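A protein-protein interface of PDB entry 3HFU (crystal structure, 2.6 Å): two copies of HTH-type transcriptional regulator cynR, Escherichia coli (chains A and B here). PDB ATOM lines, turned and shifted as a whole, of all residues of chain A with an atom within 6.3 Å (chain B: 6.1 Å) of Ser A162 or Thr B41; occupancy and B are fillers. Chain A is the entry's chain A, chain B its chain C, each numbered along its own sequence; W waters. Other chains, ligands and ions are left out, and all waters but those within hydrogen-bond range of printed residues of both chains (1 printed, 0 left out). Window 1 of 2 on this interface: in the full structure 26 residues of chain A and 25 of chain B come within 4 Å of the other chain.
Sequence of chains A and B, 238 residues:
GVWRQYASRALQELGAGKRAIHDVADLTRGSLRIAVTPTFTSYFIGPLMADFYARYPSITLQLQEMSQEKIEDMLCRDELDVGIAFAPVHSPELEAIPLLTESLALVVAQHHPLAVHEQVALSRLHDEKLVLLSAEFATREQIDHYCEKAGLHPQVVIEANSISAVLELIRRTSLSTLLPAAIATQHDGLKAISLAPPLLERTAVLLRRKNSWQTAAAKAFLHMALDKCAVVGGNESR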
ATOM      1  N   LEU A 133      15.147  23.829  -8.446  1.00  0.00           N
ATOM      2  CA  LEU A 133      13.853  23.880  -7.781  1.00  0.00           C
ATOM      3  C   LEU A 133      12.995  22.904  -8.598  1.00  0.00           C
ATOM      4  O   LEU A 133      13.287  22.643  -9.777  1.00  0.00           O
ATOM      5  CB  LEU A 133      13.237  25.297  -7.856  1.00  0.00           C
ATOM      6  CG  LEU A 133      13.733  26.426  -6.920  1.00  0.00           C
ATOM      7  CD1 LEU A 133      13.017  27.734  -7.236  1.00  0.00           C
ATOM      8  CD2 LEU A 133      13.485  26.055  -5.478  1.00  0.00           C
ATOM      9  N   SER A 134      11.948  22.357  -7.985  1.00  0.00           N
ATOM     10  CA  SER A 134      11.084  21.432  -8.708  1.00  0.00           C
ATOM     11  C   SER A 134      10.088  22.195  -9.588  1.00  0.00           C
ATOM     12  O   SER A 134       9.873  23.391  -9.404  1.00  0.00           O
ATOM     13  CB  SER A 134      10.356  20.486  -7.736  1.00  0.00           C
ATOM     14  OG  SER A 134       9.565  21.170  -6.795  1.00  0.00           O
ATOM     15  N   PHE A 137       7.787  25.365  -8.984  1.00  0.00           N
ATOM     16  CA  PHE A 137       8.231  26.750  -9.102  1.00  0.00           C
ATOM     17  C   PHE A 137       8.304  27.322 -10.504  1.00  0.00           C
ATOM     18  O   PHE A 137       8.747  26.666 -11.439  1.00  0.00           O
ATOM     19  CB  PHE A 137       9.595  26.921  -8.439  1.00  0.00           C
ATOM     20  CG  PHE A 137       9.608  26.578  -6.980  1.00  0.00           C
ATOM     21  CD1 PHE A 137       9.783  25.260  -6.563  1.00  0.00           C
ATOM     22  CD2 PHE A 137       9.434  27.571  -6.018  1.00  0.00           C
ATOM     23  CE1 PHE A 137       9.786  24.938  -5.202  1.00  0.00           C
ATOM     24  CE2 PHE A 137       9.435  27.264  -4.663  1.00  0.00           C
ATOM     25  CZ  PHE A 137       9.611  25.950  -4.247  1.00  0.00           C
ATOM     26  N   ALA A 160      14.847  20.097  -5.422  1.00  0.00           N
ATOM     27  CA  ALA A 160      14.306  20.425  -4.107  1.00  0.00           C
ATOM     28  C   ALA A 160      13.179  21.423  -4.255  1.00  0.00           C
ATOM     29  O   ALA A 160      13.131  22.155  -5.238  1.00  0.00           O
ATOM     30  CB  ALA A 160      15.399  20.995  -3.214  1.00  0.00           C
ATOM     31  N   ASN A 161      12.260  21.446  -3.294  1.00  0.00           N
ATOM     32  CA  ASN A 161      11.139  22.377  -3.365  1.00  0.00           C
ATOM     33  C   ASN A 161      11.328  23.523  -2.381  1.00  0.00           C
ATOM     34  O   ASN A 161      10.367  24.042  -1.826  1.00  0.00           O
ATOM     35  CB  ASN A 161       9.829  21.643  -3.085  1.00  0.00           C
ATOM     36  CG  ASN A 161       9.639  21.305  -1.617  1.00  0.00           C
ATOM     37  OD1 ASN A 161      10.592  20.961  -0.921  1.00  0.00           O
ATOM     38  ND2 ASN A 161       8.395  21.378  -1.146  1.00  0.00           N
ATOM     39  N   SER A 162      12.585  23.912  -2.183  1.00  0.00           N
ATOM     40  CA  SER A 162      12.951  24.993  -1.269  1.00  0.00           C
ATOM     41  C   SER A 162      14.270  25.643  -1.690  1.00  0.00           C
ATOM     42  O   SER A 162      15.278  24.959  -1.828  1.00  0.00           O
ATOM     43  CB  SER A 162      13.074  24.440   0.152  1.00  0.00           C
ATOM     44  OG  SER A 162      14.025  25.163   0.906  1.00  0.00           O
ATOM     45  N   ILE A 163      14.267  26.959  -1.889  1.00  0.00           N
ATOM     46  CA  ILE A 163      15.480  27.678  -2.295  1.00  0.00           C
ATOM     47  C   ILE A 163      16.627  27.469  -1.308  1.00  0.00           C
ATOM     48  O   ILE A 163      17.762  27.211  -1.698  1.00  0.00           O
ATOM     49  CB  ILE A 163      15.225  29.220  -2.426  1.00  0.00           C
ATOM     50  CG1 ILE A 163      14.509  29.538  -3.737  1.00  0.00           C
ATOM     51  CG2 ILE A 163      16.539  29.970  -2.418  1.00  0.00           C
ATOM     52  CD1 ILE A 163      13.180  28.846  -3.881  1.00  0.00           C
ATOM     53  N   SER A 164      16.316  27.583  -0.025  1.00  0.00           N
ATOM     54  CA  SER A 164      17.314  27.438   1.016  1.00  0.00           C
ATOM     55  C   SER A 164      18.009  26.098   0.913  1.00  0.00           C
ATOM     56  O   SER A 164      19.222  26.012   1.069  1.00  0.00           O
ATOM     57  CB  SER A 164      16.655  27.557   2.373  1.00  0.00           C
ATOM     58  OG  SER A 164      15.698  26.529   2.502  1.00  0.00           O
ATOM     59  N   ALA A 165      17.235  25.051   0.660  1.00  0.00           N
ATOM     60  CA  ALA A 165      17.791  23.703   0.536  1.00  0.00           C
ATOM     61  C   ALA A 165      18.782  23.681  -0.633  1.00  0.00           C
ATOM     62  O   ALA A 165      19.872  23.117  -0.535  1.00  0.00           O
ATOM     63  CB  ALA A 165      16.670  22.703   0.297  1.00  0.00           C
ATOM     64  N   VAL A 166      18.391  24.299  -1.739  1.00  0.00           N
ATOM     65  CA  VAL A 166      19.252  24.364  -2.904  1.00  0.00           C
ATOM     66  C   VAL A 166      20.576  25.044  -2.526  1.00  0.00           C
ATOM     67  O   VAL A 166      21.680  24.531  -2.805  1.00  0.00           O
ATOM     68  CB  VAL A 166      18.567  25.157  -4.047  1.00  0.00           C
ATOM     69  CG1 VAL A 166      19.495  25.243  -5.288  1.00  0.00           C
ATOM     70  CG2 VAL A 166      17.262  24.475  -4.416  1.00  0.00           C
ATOM     71  N   LEU A 167      20.459  26.200  -1.878  1.00  0.00           N
ATOM     72  CA  LEU A 167      21.638  26.944  -1.475  1.00  0.00           C
ATOM     73  C   LEU A 167      22.485  26.109  -0.529  1.00  0.00           C
ATOM     74  O   LEU A 167      23.708  26.072  -0.664  1.00  0.00           O
ATOM     75  CB  LEU A 167      21.247  28.269  -0.799  1.00  0.00           C
ATOM     76  CG  LEU A 167      20.507  29.311  -1.659  1.00  0.00           C
ATOM     77  CD1 LEU A 167      20.345  30.603  -0.863  1.00  0.00           C
ATOM     78  CD2 LEU A 167      21.269  29.566  -2.965  1.00  0.00           C
ATOM     79  N   GLU A 168      21.834  25.422   0.413  1.00  0.00           N
ATOM     80  CA  GLU A 168      22.544  24.605   1.394  1.00  0.00           C
ATOM     81  C   GLU A 168      23.363  23.530   0.690  1.00  0.00           C
ATOM     82  O   GLU A 168      24.540  23.346   0.966  1.00  0.00           O
ATOM     83  CB  GLU A 168      21.556  23.954   2.357  1.00  0.00           C
ATOM     84  CG  GLU A 168      22.231  23.320   3.552  1.00  0.00           C
ATOM     85  CD  GLU A 168      22.908  24.348   4.434  1.00  0.00           C
ATOM     86  OE1 GLU A 168      22.189  25.213   4.981  1.00  0.00           O
ATOM     87  OE2 GLU A 168      24.151  24.295   4.576  1.00  0.00           O
ATOM     88  N   VAL B  36      10.631  15.863   4.214  1.00  0.00           N
ATOM     89  CA  VAL B  36      10.818  16.201   5.615  1.00  0.00           C
ATOM     90  C   VAL B  36       9.875  17.323   5.996  1.00  0.00           C
ATOM     91  O   VAL B  36       9.364  18.048   5.127  1.00  0.00           O
ATOM     92  CB  VAL B  36      12.261  16.696   5.905  1.00  0.00           C
ATOM     93  CG1 VAL B  36      13.262  15.561   5.728  1.00  0.00           C
ATOM     94  CG2 VAL B  36      12.606  17.867   4.977  1.00  0.00           C
ATOM     95  N   THR B  37       9.653  17.462   7.303  1.00  0.00           N
ATOM     96  CA  THR B  37       8.807  18.517   7.839  1.00  0.00           C
ATOM     97  C   THR B  37       9.680  19.791   7.778  1.00  0.00           C
ATOM     98  O   THR B  37      10.907  19.716   7.849  1.00  0.00           O
ATOM     99  CB  THR B  37       8.314  18.163   9.305  1.00  0.00           C
ATOM    100  OG1 THR B  37       9.387  17.594  10.067  1.00  0.00           O
ATOM    101  CG2 THR B  37       7.165  17.147   9.281  1.00  0.00           C
ATOM    102  N   PRO B  38       9.061  20.971   7.615  1.00  0.00           N
ATOM    103  CA  PRO B  38       9.752  22.265   7.522  1.00  0.00           C
ATOM    104  C   PRO B  38      11.035  22.518   8.313  1.00  0.00           C
ATOM    105  O   PRO B  38      12.035  22.946   7.739  1.00  0.00           O
ATOM    106  CB  PRO B  38       8.658  23.260   7.883  1.00  0.00           C
ATOM    107  CG  PRO B  38       7.459  22.628   7.287  1.00  0.00           C
ATOM    108  CD  PRO B  38       7.605  21.177   7.702  1.00  0.00           C
ATOM    109  N   THR B  39      11.022  22.269   9.616  1.00  0.00           N
ATOM    110  CA  THR B  39      12.218  22.534  10.421  1.00  0.00           C
ATOM    111  C   THR B  39      13.510  21.772  10.045  1.00  0.00           C
ATOM    112  O   THR B  39      14.617  22.288  10.243  1.00  0.00           O
ATOM    113  CB  THR B  39      11.951  22.313  11.948  1.00  0.00           C
ATOM    114  OG1 THR B  39      11.534  20.958  12.180  1.00  0.00           O
ATOM    115  CG2 THR B  39      10.875  23.304  12.472  1.00  0.00           C
ATOM    116  N   PHE B  40      13.385  20.565   9.497  1.00  0.00           N
ATOM    117  CA  PHE B  40      14.578  19.803   9.158  1.00  0.00           C
ATOM    118  C   PHE B  40      15.306  20.370   7.979  1.00  0.00           C
ATOM    119  O   PHE B  40      16.503  20.154   7.820  1.00  0.00           O
ATOM    120  CB  PHE B  40      14.232  18.347   8.898  1.00  0.00           C
ATOM    121  CG  PHE B  40      13.732  17.632  10.111  1.00  0.00           C
ATOM    122  CD1 PHE B  40      12.365  17.530  10.363  1.00  0.00           C
ATOM    123  CD2 PHE B  40      14.630  17.088  11.030  1.00  0.00           C
ATOM    124  CE1 PHE B  40      11.893  16.891  11.519  1.00  0.00           C
ATOM    125  CE2 PHE B  40      14.176  16.453  12.184  1.00  0.00           C
ATOM    126  CZ  PHE B  40      12.802  16.352  12.431  1.00  0.00           C
ATOM    127  N   THR B  41      14.579  21.115   7.163  1.00  0.00           N
ATOM    128  CA  THR B  41      15.164  21.718   5.991  1.00  0.00           C
ATOM    129  C   THR B  41      16.186  22.776   6.376  1.00  0.00           C
ATOM    130  O   THR B  41      17.176  22.974   5.672  1.00  0.00           O
ATOM    131  CB  THR B  41      14.093  22.380   5.148  1.00  0.00           C
ATOM    132  OG1 THR B  41      13.014  21.465   4.968  1.00  0.00           O
ATOM    133  CG2 THR B  41      14.649  22.772   3.799  1.00  0.00           C
ATOM    134  N   SER B  42      15.954  23.443   7.504  1.00  0.00           N
ATOM    135  CA  SER B  42      16.835  24.513   7.958  1.00  0.00           C
ATOM    136  C   SER B  42      18.083  24.127   8.755  1.00  0.00           C
ATOM    137  O   SER B  42      18.761  25.002   9.286  1.00  0.00           O
ATOM    138  CB  SER B  42      16.024  25.520   8.767  1.00  0.00           C
ATOM    139  OG  SER B  42      14.890  25.948   8.040  1.00  0.00           O
ATOM    140  N   TYR B  43      18.400  22.842   8.856  1.00  0.00           N
ATOM    141  CA  TYR B  43      19.588  22.473   9.601  1.00  0.00           C
ATOM    142  C   TYR B  43      20.021  21.037   9.462  1.00  0.00           C
ATOM    143  O   TYR B  43      21.213  20.744   9.481  1.00  0.00           O
ATOM    144  CB  TYR B  43      19.396  22.796  11.082  1.00  0.00           C
ATOM    145  CG  TYR B  43      18.547  21.823  11.880  1.00  0.00           C
ATOM    146  CD1 TYR B  43      19.079  20.616  12.358  1.00  0.00           C
ATOM    147  CD2 TYR B  43      17.234  22.133  12.217  1.00  0.00           C
ATOM    148  CE1 TYR B  43      18.319  19.754  13.155  1.00  0.00           C
ATOM    149  CE2 TYR B  43      16.470  21.277  13.015  1.00  0.00           C
ATOM    150  CZ  TYR B  43      17.017  20.093  13.480  1.00  0.00           C
ATOM    151  OH  TYR B  43      16.257  19.261  14.279  1.00  0.00           O
ATOM    152  N   PHE B  44      19.056  20.141   9.310  1.00  0.00           N
ATOM    153  CA  PHE B  44      19.354  18.714   9.219  1.00  0.00           C
ATOM    154  C   PHE B  44      19.652  18.150   7.824  1.00  0.00           C
ATOM    155  O   PHE B  44      20.787  17.768   7.516  1.00  0.00           O
ATOM    156  CB  PHE B  44      18.195  17.924   9.829  1.00  0.00           C
ATOM    157  CG  PHE B  44      18.497  16.473  10.036  1.00  0.00           C
ATOM    158  CD1 PHE B  44      19.236  16.051  11.142  1.00  0.00           C
ATOM    159  CD2 PHE B  44      18.078  15.523   9.111  1.00  0.00           C
ATOM    160  CE1 PHE B  44      19.555  14.709  11.330  1.00  0.00           C
ATOM    161  CE2 PHE B  44      18.392  14.168   9.286  1.00  0.00           C
ATOM    162  CZ  PHE B  44      19.134  13.766  10.402  1.00  0.00           C
ATOM    163  N   ILE B  45      18.609  18.119   6.994  1.00  0.00           N
ATOM    164  CA  ILE B  45      18.641  17.561   5.651  1.00  0.00           C
ATOM    165  C   ILE B  45      19.725  18.062   4.683  1.00  0.00           C
ATOM    166  O   ILE B  45      20.288  17.280   3.910  1.00  0.00           O
ATOM    167  CB  ILE B  45      17.248  17.707   5.017  1.00  0.00           C
ATOM    168  CG1 ILE B  45      17.057  16.621   3.960  1.00  0.00           C
ATOM    169  CG2 ILE B  45      17.077  19.098   4.456  1.00  0.00           C
ATOM    170  CD1 ILE B  45      17.320  15.184   4.490  1.00  0.00           C
ATOM    171  N   GLY B  46      20.021  19.355   4.742  1.00  0.00           N
ATOM    172  CA  GLY B  46      21.025  19.930   3.869  1.00  0.00           C
ATOM    173  C   GLY B  46      22.369  19.230   3.972  1.00  0.00           C
ATOM    174  O   GLY B  46      22.850  18.670   2.989  1.00  0.00           O
ATOM    175  N   LEU B  63      14.184  16.081  -3.010  1.00  0.00           N
ATOM    176  CA  LEU B  63      13.886  16.575  -1.663  1.00  0.00           C
ATOM    177  C   LEU B  63      12.640  17.473  -1.634  1.00  0.00           C
ATOM    178  O   LEU B  63      12.510  18.411  -2.417  1.00  0.00           O
ATOM    179  CB  LEU B  63      15.100  17.340  -1.127  1.00  0.00           C
ATOM    180  CG  LEU B  63      15.155  17.892   0.305  1.00  0.00           C
ATOM    181  CD1 LEU B  63      14.170  19.029   0.461  1.00  0.00           C
ATOM    182  CD2 LEU B  63      14.874  16.786   1.312  1.00  0.00           C
ATOM    183  N   GLN B  64      11.716  17.182  -0.730  1.00  0.00           N
ATOM    184  CA  GLN B  64      10.509  17.990  -0.618  1.00  0.00           C
ATOM    185  C   GLN B  64      10.149  18.187   0.839  1.00  0.00           C
ATOM    186  O   GLN B  64      10.138  17.238   1.618  1.00  0.00           O
ATOM    187  CB  GLN B  64       9.335  17.323  -1.311  1.00  0.00           C
ATOM    188  CG  GLN B  64       9.589  16.928  -2.728  1.00  0.00           C
ATOM    189  CD  GLN B  64       8.423  16.159  -3.289  1.00  0.00           C
ATOM    190  OE1 GLN B  64       7.371  16.729  -3.594  1.00  0.00           O
ATOM    191  NE2 GLN B  64       8.590  14.846  -3.406  1.00  0.00           N
ATOM    192  N   GLU B  65       9.862  19.422   1.217  1.00  0.00           N
ATOM    193  CA  GLU B  65       9.482  19.670   2.583  1.00  0.00           C
ATOM    194  C   GLU B  65       7.972  19.830   2.565  1.00  0.00           C
ATOM    195  O   GLU B  65       7.422  20.482   1.676  1.00  0.00           O
ATOM    196  CB  GLU B  65      10.169  20.923   3.113  1.00  0.00           C
ATOM    197  CG  GLU B  65       9.838  22.207   2.394  1.00  0.00           C
ATOM    198  CD  GLU B  65      10.451  23.406   3.090  1.00  0.00           C
ATOM    199  OE1 GLU B  65      10.360  24.526   2.545  1.00  0.00           O
ATOM    200  OE2 GLU B  65      11.025  23.231   4.189  1.00  0.00           O
ATOM    201  N   ILE B 183      18.804  25.185  14.481  1.00  0.00           N
ATOM    202  CA  ILE B 183      18.727  26.160  13.384  1.00  0.00           C
ATOM    203  C   ILE B 183      19.751  27.285  13.569  1.00  0.00           C
ATOM    204  O   ILE B 183      20.326  27.786  12.598  1.00  0.00           O
ATOM    205  CB  ILE B 183      17.309  26.854  13.317  1.00  0.00           C
ATOM    206  CG1 ILE B 183      16.188  25.825  13.153  1.00  0.00           C
ATOM    207  CG2 ILE B 183      17.264  27.867  12.177  1.00  0.00           C
ATOM    208  CD1 ILE B 183      16.014  25.316  11.762  1.00  0.00           C
HETATM  209  O   HOH W   1       8.645  24.968  -0.224  1.00  0.00           O
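No position is printed for both chains.
CA of Ala A160 touches O of Leu B63, at 3.2 Å.
Asn A161 touches Gln B64 (OD1 to CA, 3.0 Å).
Ser A162 touches Thr B41 (OG to CG2, 3.8 Å).
Ser A162 touches Glu B65 (CB to OE1, 3.6 Å).
Glu A168 touches Gly B46 (CG to CA, 3.6 Å).
The backbone carbonyl oxygen (O) of Ala A160 is in hydrogen-bond range of the backbone NH (N) of Ser A134.
The side-chain hydroxyl (OG) of Ser A164 is in hydrogen-bond range of the side-chain hydroxyl (OG) of Ser A162 (2.7 Å).
The backbone NH (N) of Ala A165 is in hydrogen-bond range of the side-chain hydroxyl (OG) of Ser A162, at 3.2 Å.
The backbone carbonyl oxygen of Gln B64 lies within hydrogen-bond range of the backbone NH of Val B36 (3.0 Å).
OG1 of Thr B41 lies within hydrogen-bond range of O of Pro B38, at 3.3 Å.
OG1 of Thr B41 is in hydrogen-bond range of OE2 of Glu B65, at 2.8 Å.
Water W1 lies within hydrogen-bond range of the backbone carbonyl oxygen (O) of Asn A161 and the side-chain carboxylate (OE1) of Glu B65.
The backbone NH of Asn A161 is in hydrogen-bond range of the backbone carbonyl oxygen of Leu B63.
OD1 of Asn A161 sits at hydrogen-bond distance from N of Glu B65 (2.7 Å).
Printed residues of chain B within 4 Å of Ala A160: Leu B63.
Printed residues of chain B within 4 Å of Asn A161: Leu B63 (3.2 Å), Gln B64 (3.0 Å) and Glu B65 (2.7 Å).
Of chain B, only Thr B41 (3.8 Å) and Glu B65 (3.6 Å) come within 4 Å of Ser A162.
Val A166 touches none of the printed residues of chain B.
Of the printed residues of chain A, Leu B63 touches Ala A160 and Asn A161.
The nearest residue of chain A that does not touch Thr B41 is Ala A165 (4.04 Å).
The nearest printed residue of chain A that does not touch Gly B46 is Ala A165 (5.6 Å).
Of the 12 printed residues of chain A, 4 touch a printed residue of chain B.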
